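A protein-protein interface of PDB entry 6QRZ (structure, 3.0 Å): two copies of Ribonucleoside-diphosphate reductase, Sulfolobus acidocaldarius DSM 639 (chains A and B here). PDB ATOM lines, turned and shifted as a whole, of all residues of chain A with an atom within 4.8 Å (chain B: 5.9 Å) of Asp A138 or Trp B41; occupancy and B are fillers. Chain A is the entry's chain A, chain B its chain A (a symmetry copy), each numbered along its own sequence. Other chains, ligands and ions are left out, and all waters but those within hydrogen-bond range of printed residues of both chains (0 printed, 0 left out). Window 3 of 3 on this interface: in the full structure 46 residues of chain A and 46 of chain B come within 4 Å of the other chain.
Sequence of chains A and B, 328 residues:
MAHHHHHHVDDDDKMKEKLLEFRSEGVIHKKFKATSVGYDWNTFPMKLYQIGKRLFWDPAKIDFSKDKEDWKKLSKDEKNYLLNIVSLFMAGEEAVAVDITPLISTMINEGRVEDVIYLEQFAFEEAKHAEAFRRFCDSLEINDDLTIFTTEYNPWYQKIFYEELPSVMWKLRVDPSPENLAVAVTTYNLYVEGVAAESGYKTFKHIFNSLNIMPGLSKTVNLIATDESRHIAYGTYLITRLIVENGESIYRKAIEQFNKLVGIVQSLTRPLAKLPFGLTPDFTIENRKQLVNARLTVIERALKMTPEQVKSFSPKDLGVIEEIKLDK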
ATOM      1  N   GLU A 131      12.725   6.000 -20.688  1.00  0.00           N
ATOM      2  CA  GLU A 131      11.654   6.430 -19.801  1.00  0.00           C
ATOM      3  C   GLU A 131      10.306   5.893 -20.263  1.00  0.00           C
ATOM      4  O   GLU A 131       9.500   5.437 -19.445  1.00  0.00           O
ATOM      5  CB  GLU A 131      11.620   7.955 -19.719  1.00  0.00           C
ATOM      6  CG  GLU A 131      10.437   8.496 -18.939  1.00  0.00           C
ATOM      7  CD  GLU A 131      10.318  10.001 -19.029  1.00  0.00           C
ATOM      8  OE1 GLU A 131      10.721  10.570 -20.066  1.00  0.00           O
ATOM      9  OE2 GLU A 131       9.824  10.616 -18.060  1.00  0.00           O
ATOM     10  N   ARG A 134       9.864   2.199 -19.394  1.00  0.00           N
ATOM     11  CA  ARG A 134       9.664   2.099 -17.952  1.00  0.00           C
ATOM     12  C   ARG A 134       8.318   2.683 -17.541  1.00  0.00           C
ATOM     13  O   ARG A 134       7.708   2.213 -16.573  1.00  0.00           O
ATOM     14  CB  ARG A 134      10.805   2.803 -17.217  1.00  0.00           C
ATOM     15  CG  ARG A 134      10.887   2.492 -15.730  1.00  0.00           C
ATOM     16  CD  ARG A 134      11.205   1.026 -15.481  1.00  0.00           C
ATOM     17  NE  ARG A 134      10.021   0.258 -15.109  1.00  0.00           N
ATOM     18  CZ  ARG A 134      10.036  -1.039 -14.813  1.00  0.00           C
ATOM     19  NH1 ARG A 134      11.176  -1.716 -14.849  1.00  0.00           N
ATOM     20  NH2 ARG A 134       8.912  -1.659 -14.482  1.00  0.00           N
ATOM     21  N   ARG A 135       7.839   3.699 -18.262  1.00  0.00           N
ATOM     22  CA  ARG A 135       6.496   4.211 -18.014  1.00  0.00           C
ATOM     23  C   ARG A 135       5.437   3.196 -18.425  1.00  0.00           C
ATOM     24  O   ARG A 135       4.447   2.997 -17.710  1.00  0.00           O
ATOM     25  CB  ARG A 135       6.288   5.532 -18.756  1.00  0.00           C
ATOM     26  CG  ARG A 135       6.954   6.731 -18.101  1.00  0.00           C
ATOM     27  CD  ARG A 135       6.421   6.953 -16.699  1.00  0.00           C
ATOM     28  NE  ARG A 135       6.984   8.149 -16.082  1.00  0.00           N
ATOM     29  CZ  ARG A 135       6.685   8.566 -14.856  1.00  0.00           C
ATOM     30  NH1 ARG A 135       5.828   7.883 -14.110  1.00  0.00           N
ATOM     31  NH2 ARG A 135       7.246   9.666 -14.375  1.00  0.00           N
ATOM     32  N   PHE A 136       5.626   2.547 -19.577  1.00  0.00           N
ATOM     33  CA  PHE A 136       4.691   1.515 -20.011  1.00  0.00           C
ATOM     34  C   PHE A 136       4.733   0.302 -19.094  1.00  0.00           C
ATOM     35  O   PHE A 136       3.698  -0.332 -18.858  1.00  0.00           O
ATOM     36  CB  PHE A 136       4.994   1.104 -21.452  1.00  0.00           C
ATOM     37  CG  PHE A 136       4.181  -0.063 -21.933  1.00  0.00           C
ATOM     38  CD1 PHE A 136       2.845   0.095 -22.256  1.00  0.00           C
ATOM     39  CD2 PHE A 136       4.754  -1.318 -22.067  1.00  0.00           C
ATOM     40  CE1 PHE A 136       2.091  -0.975 -22.701  1.00  0.00           C
ATOM     41  CE2 PHE A 136       4.007  -2.393 -22.513  1.00  0.00           C
ATOM     42  CZ  PHE A 136       2.674  -2.220 -22.831  1.00  0.00           C
ATOM     43  N   CYS A 137       5.912  -0.033 -18.566  1.00  0.00           N
ATOM     44  CA  CYS A 137       6.006  -1.150 -17.633  1.00  0.00           C
ATOM     45  C   CYS A 137       5.341  -0.816 -16.304  1.00  0.00           C
ATOM     46  O   CYS A 137       4.609  -1.642 -15.746  1.00  0.00           O
ATOM     47  CB  CYS A 137       7.467  -1.537 -17.416  1.00  0.00           C
ATOM     48  SG  CYS A 137       8.290  -2.232 -18.861  1.00  0.00           S
ATOM     49  N   ASP A 138       5.582   0.389 -15.781  1.00  0.00           N
ATOM     50  CA  ASP A 138       4.936   0.783 -14.535  1.00  0.00           C
ATOM     51  C   ASP A 138       3.431   0.948 -14.706  1.00  0.00           C
ATOM     52  O   ASP A 138       2.684   0.838 -13.726  1.00  0.00           O
ATOM     53  CB  ASP A 138       5.555   2.076 -14.003  1.00  0.00           C
ATOM     54  CG  ASP A 138       6.971   1.885 -13.517  1.00  0.00           C
ATOM     55  OD1 ASP A 138       7.291   0.774 -13.047  1.00  0.00           O
ATOM     56  OD2 ASP A 138       7.766   2.843 -13.609  1.00  0.00           O
ATOM     57  N   SER A 139       2.968   1.217 -15.930  1.00  0.00           N
ATOM     58  CA  SER A 139       1.533   1.345 -16.162  1.00  0.00           C
ATOM     59  C   SER A 139       0.838  -0.009 -16.126  1.00  0.00           C
ATOM     60  O   SER A 139      -0.363  -0.080 -15.840  1.00  0.00           O
ATOM     61  CB  SER A 139       1.273   2.037 -17.501  1.00  0.00           C
ATOM     62  OG  SER A 139       1.750   1.254 -18.581  1.00  0.00           O
ATOM     63  N   LEU A 140       1.568  -1.087 -16.415  1.00  0.00           N
ATOM     64  CA  LEU A 140       1.039  -2.442 -16.353  1.00  0.00           C
ATOM     65  C   LEU A 140       1.269  -3.097 -14.997  1.00  0.00           C
ATOM     66  O   LEU A 140       1.200  -4.329 -14.898  1.00  0.00           O
ATOM     67  CB  LEU A 140       1.658  -3.310 -17.453  1.00  0.00           C
ATOM     68  CG  LEU A 140       1.496  -2.860 -18.904  1.00  0.00           C
ATOM     69  CD1 LEU A 140       2.172  -3.854 -19.829  1.00  0.00           C
ATOM     70  CD2 LEU A 140       0.031  -2.685 -19.273  1.00  0.00           C
ATOM     71  N   GLU A 141       1.554  -2.302 -13.962  1.00  0.00           N
ATOM     72  CA  GLU A 141       1.738  -2.790 -12.598  1.00  0.00           C
ATOM     73  C   GLU A 141       2.998  -3.642 -12.496  1.00  0.00           C
ATOM     74  O   GLU A 141       3.295  -4.195 -11.432  1.00  0.00           O
ATOM     75  CB  GLU A 141       0.508  -3.580 -12.125  1.00  0.00           C
ATOM     76  CG  GLU A 141       0.398  -3.721 -10.610  1.00  0.00           C
ATOM     77  CD  GLU A 141      -0.740  -4.616 -10.165  1.00  0.00           C
ATOM     78  OE1 GLU A 141      -1.563  -5.026 -11.013  1.00  0.00           O
ATOM     79  OE2 GLU A 141      -0.801  -4.910  -8.953  1.00  0.00           O
ATOM     80  N   ILE A 142       3.745  -3.752 -13.595  1.00  0.00           N
ATOM     81  CA  ILE A 142       4.957  -4.562 -13.635  1.00  0.00           C
ATOM     82  C   ILE A 142       5.982  -3.967 -12.682  1.00  0.00           C
ATOM     83  O   ILE A 142       6.666  -2.992 -13.013  1.00  0.00           O
ATOM     84  CB  ILE A 142       5.523  -4.664 -15.063  1.00  0.00           C
ATOM     85  CG1 ILE A 142       4.469  -5.228 -16.019  1.00  0.00           C
ATOM     86  CG2 ILE A 142       6.771  -5.540 -15.080  1.00  0.00           C
ATOM     87  CD1 ILE A 142       4.886  -5.200 -17.468  1.00  0.00           C
ATOM     88  N   TYR B  39      13.912   2.760 -12.214  1.00  0.00           N
ATOM     89  CA  TYR B  39      14.112   4.198 -12.106  1.00  0.00           C
ATOM     90  C   TYR B  39      13.398   4.736 -10.874  1.00  0.00           C
ATOM     91  O   TYR B  39      12.260   4.356 -10.586  1.00  0.00           O
ATOM     92  CB  TYR B  39      13.598   4.919 -13.354  1.00  0.00           C
ATOM     93  CG  TYR B  39      14.414   4.680 -14.605  1.00  0.00           C
ATOM     94  CD1 TYR B  39      15.714   4.198 -14.531  1.00  0.00           C
ATOM     95  CD2 TYR B  39      13.885   4.945 -15.861  1.00  0.00           C
ATOM     96  CE1 TYR B  39      16.463   3.982 -15.673  1.00  0.00           C
ATOM     97  CE2 TYR B  39      14.625   4.732 -17.009  1.00  0.00           C
ATOM     98  CZ  TYR B  39      15.912   4.252 -16.910  1.00  0.00           C
ATOM     99  OH  TYR B  39      16.653   4.039 -18.049  1.00  0.00           O
ATOM    100  N   ASP B  40      14.073   5.629 -10.151  1.00  0.00           N
ATOM    101  CA  ASP B  40      13.491   6.300  -8.990  1.00  0.00           C
ATOM    102  C   ASP B  40      12.842   7.593  -9.469  1.00  0.00           C
ATOM    103  O   ASP B  40      13.509   8.622  -9.610  1.00  0.00           O
ATOM    104  CB  ASP B  40      14.551   6.566  -7.928  1.00  0.00           C
ATOM    105  CG  ASP B  40      15.123   5.291  -7.341  1.00  0.00           C
ATOM    106  OD1 ASP B  40      14.392   4.280  -7.283  1.00  0.00           O
ATOM    107  OD2 ASP B  40      16.305   5.301  -6.938  1.00  0.00           O
ATOM    108  N   TRP B  41      11.531   7.542  -9.716  1.00  0.00           N
ATOM    109  CA  TRP B  41      10.831   8.692 -10.277  1.00  0.00           C
ATOM    110  C   TRP B  41      10.696   9.840  -9.288  1.00  0.00           C
ATOM    111  O   TRP B  41      10.507  10.984  -9.713  1.00  0.00           O
ATOM    112  CB  TRP B  41       9.448   8.272 -10.773  1.00  0.00           C
ATOM    113  CG  TRP B  41       9.485   7.180 -11.796  1.00  0.00           C
ATOM    114  CD1 TRP B  41       9.210   5.858 -11.595  1.00  0.00           C
ATOM    115  CD2 TRP B  41       9.827   7.313 -13.179  1.00  0.00           C
ATOM    116  NE1 TRP B  41       9.354   5.162 -12.770  1.00  0.00           N
ATOM    117  CE2 TRP B  41       9.733   6.032 -13.758  1.00  0.00           C
ATOM    118  CE3 TRP B  41      10.202   8.392 -13.986  1.00  0.00           C
ATOM    119  CZ2 TRP B  41       9.999   5.801 -15.105  1.00  0.00           C
ATOM    120  CZ3 TRP B  41      10.465   8.159 -15.324  1.00  0.00           C
ATOM    121  CH2 TRP B  41      10.364   6.874 -15.868  1.00  0.00           C
ATOM    122  N   ASN B  42      10.786   9.568  -7.985  1.00  0.00           N
ATOM    123  CA  ASN B  42      10.646  10.623  -6.992  1.00  0.00           C
ATOM    124  C   ASN B  42      11.938  11.390  -6.743  1.00  0.00           C
ATOM    125  O   ASN B  42      11.918  12.375  -5.997  1.00  0.00           O
ATOM    126  CB  ASN B  42      10.132  10.044  -5.668  1.00  0.00           C
ATOM    127  CG  ASN B  42      11.052   8.980  -5.095  1.00  0.00           C
ATOM    128  OD1 ASN B  42      12.086   8.652  -5.677  1.00  0.00           O
ATOM    129  ND2 ASN B  42      10.679   8.440  -3.940  1.00  0.00           N
ATOM    130  N   THR B  43      13.052  10.968  -7.336  1.00  0.00           N
ATOM    131  CA  THR B  43      14.311  11.660  -7.118  1.00  0.00           C
ATOM    132  C   THR B  43      14.315  13.011  -7.829  1.00  0.00           C
ATOM    133  O   THR B  43      13.597  13.237  -8.808  1.00  0.00           O
ATOM    134  CB  THR B  43      15.489  10.813  -7.598  1.00  0.00           C
ATOM    135  OG1 THR B  43      15.196  10.272  -8.892  1.00  0.00           O
ATOM    136  CG2 THR B  43      15.763   9.681  -6.620  1.00  0.00           C
ATOM    137  N   MET B  46      15.103  13.223 -11.624  1.00  0.00           N
ATOM    138  CA  MET B  46      14.031  12.728 -12.479  1.00  0.00           C
ATOM    139  C   MET B  46      12.835  13.672 -12.501  1.00  0.00           C
ATOM    140  O   MET B  46      12.129  13.745 -13.513  1.00  0.00           O
ATOM    141  CB  MET B  46      13.599  11.335 -12.024  1.00  0.00           C
ATOM    142  CG  MET B  46      14.709  10.299 -12.092  1.00  0.00           C
ATOM    143  SD  MET B  46      15.233   9.914 -13.772  1.00  0.00           S
ATOM    144  CE  MET B  46      13.750   9.142 -14.412  1.00  0.00           C
ATOM    145  N   LYS B  47      12.593  14.401 -11.409  1.00  0.00           N
ATOM    146  CA  LYS B  47      11.477  15.342 -11.382  1.00  0.00           C
ATOM    147  C   LYS B  47      11.774  16.574 -12.227  1.00  0.00           C
ATOM    148  O   LYS B  47      10.873  17.121 -12.875  1.00  0.00           O
ATOM    149  CB  LYS B  47      11.149  15.729  -9.940  1.00  0.00           C
ATOM    150  CG  LYS B  47      10.541  14.590  -9.136  1.00  0.00           C
ATOM    151  CD  LYS B  47      10.052  15.051  -7.775  1.00  0.00           C
ATOM    152  CE  LYS B  47      11.206  15.461  -6.877  1.00  0.00           C
ATOM    153  NZ  LYS B  47      10.741  15.791  -5.501  1.00  0.00           N
ATOM    154  N   TYR B  49      13.682  16.237 -14.781  1.00  0.00           N
ATOM    155  CA  TYR B  49      13.627  15.633 -16.107  1.00  0.00           C
ATOM    156  C   TYR B  49      12.216  15.667 -16.675  1.00  0.00           C
ATOM    157  O   TYR B  49      12.039  15.725 -17.898  1.00  0.00           O
ATOM    158  CB  TYR B  49      14.153  14.198 -16.040  1.00  0.00           C
ATOM    159  CG  TYR B  49      14.212  13.478 -17.367  1.00  0.00           C
ATOM    160  CD1 TYR B  49      15.243  13.720 -18.265  1.00  0.00           C
ATOM    161  CD2 TYR B  49      13.249  12.541 -17.714  1.00  0.00           C
ATOM    162  CE1 TYR B  49      15.304  13.061 -19.476  1.00  0.00           C
ATOM    163  CE2 TYR B  49      13.304  11.874 -18.922  1.00  0.00           C
ATOM    164  CZ  TYR B  49      14.333  12.138 -19.798  1.00  0.00           C
ATOM    165  OH  TYR B  49      14.391  11.478 -21.002  1.00  0.00           O
ATOM    166  N   GLN B  50      11.201  15.634 -15.809  1.00  0.00           N
ATOM    167  CA  GLN B  50       9.823  15.751 -16.273  1.00  0.00           C
ATOM    168  C   GLN B  50       9.517  17.172 -16.724  1.00  0.00           C
ATOM    169  O   GLN B  50       8.966  17.386 -17.810  1.00  0.00           O
ATOM    170  CB  GLN B  50       8.855  15.324 -15.170  1.00  0.00           C
ATOM    171  CG  GLN B  50       8.933  13.859 -14.785  1.00  0.00           C
ATOM    172  CD  GLN B  50       7.972  13.512 -13.664  1.00  0.00           C
ATOM    173  OE1 GLN B  50       7.228  14.367 -13.183  1.00  0.00           O
ATOM    174  NE2 GLN B  50       7.985  12.254 -13.240  1.00  0.00           N
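The guanidinium group (NH2) of Arg A135 sits close to the side-chain amide nitrogen (NE2) of Gln B50 (2.9 Å). OD2 of Asp A138 lies close to NE1 of Trp B41 (2.9 Å).
Among the printed residues, no Asp or Glu carboxylate lies within 4 Å of a Lys or Arg side-chain nitrogen of the other chain.
CG of Glu A131 touches CH2 of Trp B41 (3.5 Å). Glu A131 touches Tyr B49 (OE1 to CE2, 3.1 Å). CG of Arg A134 touches CD2 of Tyr B39, at 3.9 Å. CG of Arg A134 touches CZ2 of Trp B41, at 3.5 Å. Arg A135 touches Trp B41 (NH2 to CE3, 3.2 Å).
No position is printed for both chains. Of the 7 pairs that touch across the chains among the printed residues, none has its exchanged pair printed and touching as well.
Of chain B, only Trp B41 (2.9 Å) comes within 4 Å of Asp A138. Trp B41 touches four residues of chain A. Of the printed residues of chain B, Glu A131 touches Trp B41 and Tyr B49. Printed residues of chain B within 4 Å of Arg A135: Trp B41 (3.2 Å) and Gln B50 (2.9 Å). Of the printed residues of chain A, Gln B50 touches Arg A135 (2.9 Å). Asp B40 touches none of the printed residues of chain A. Ile A142 touches none of the printed residues of chain B.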
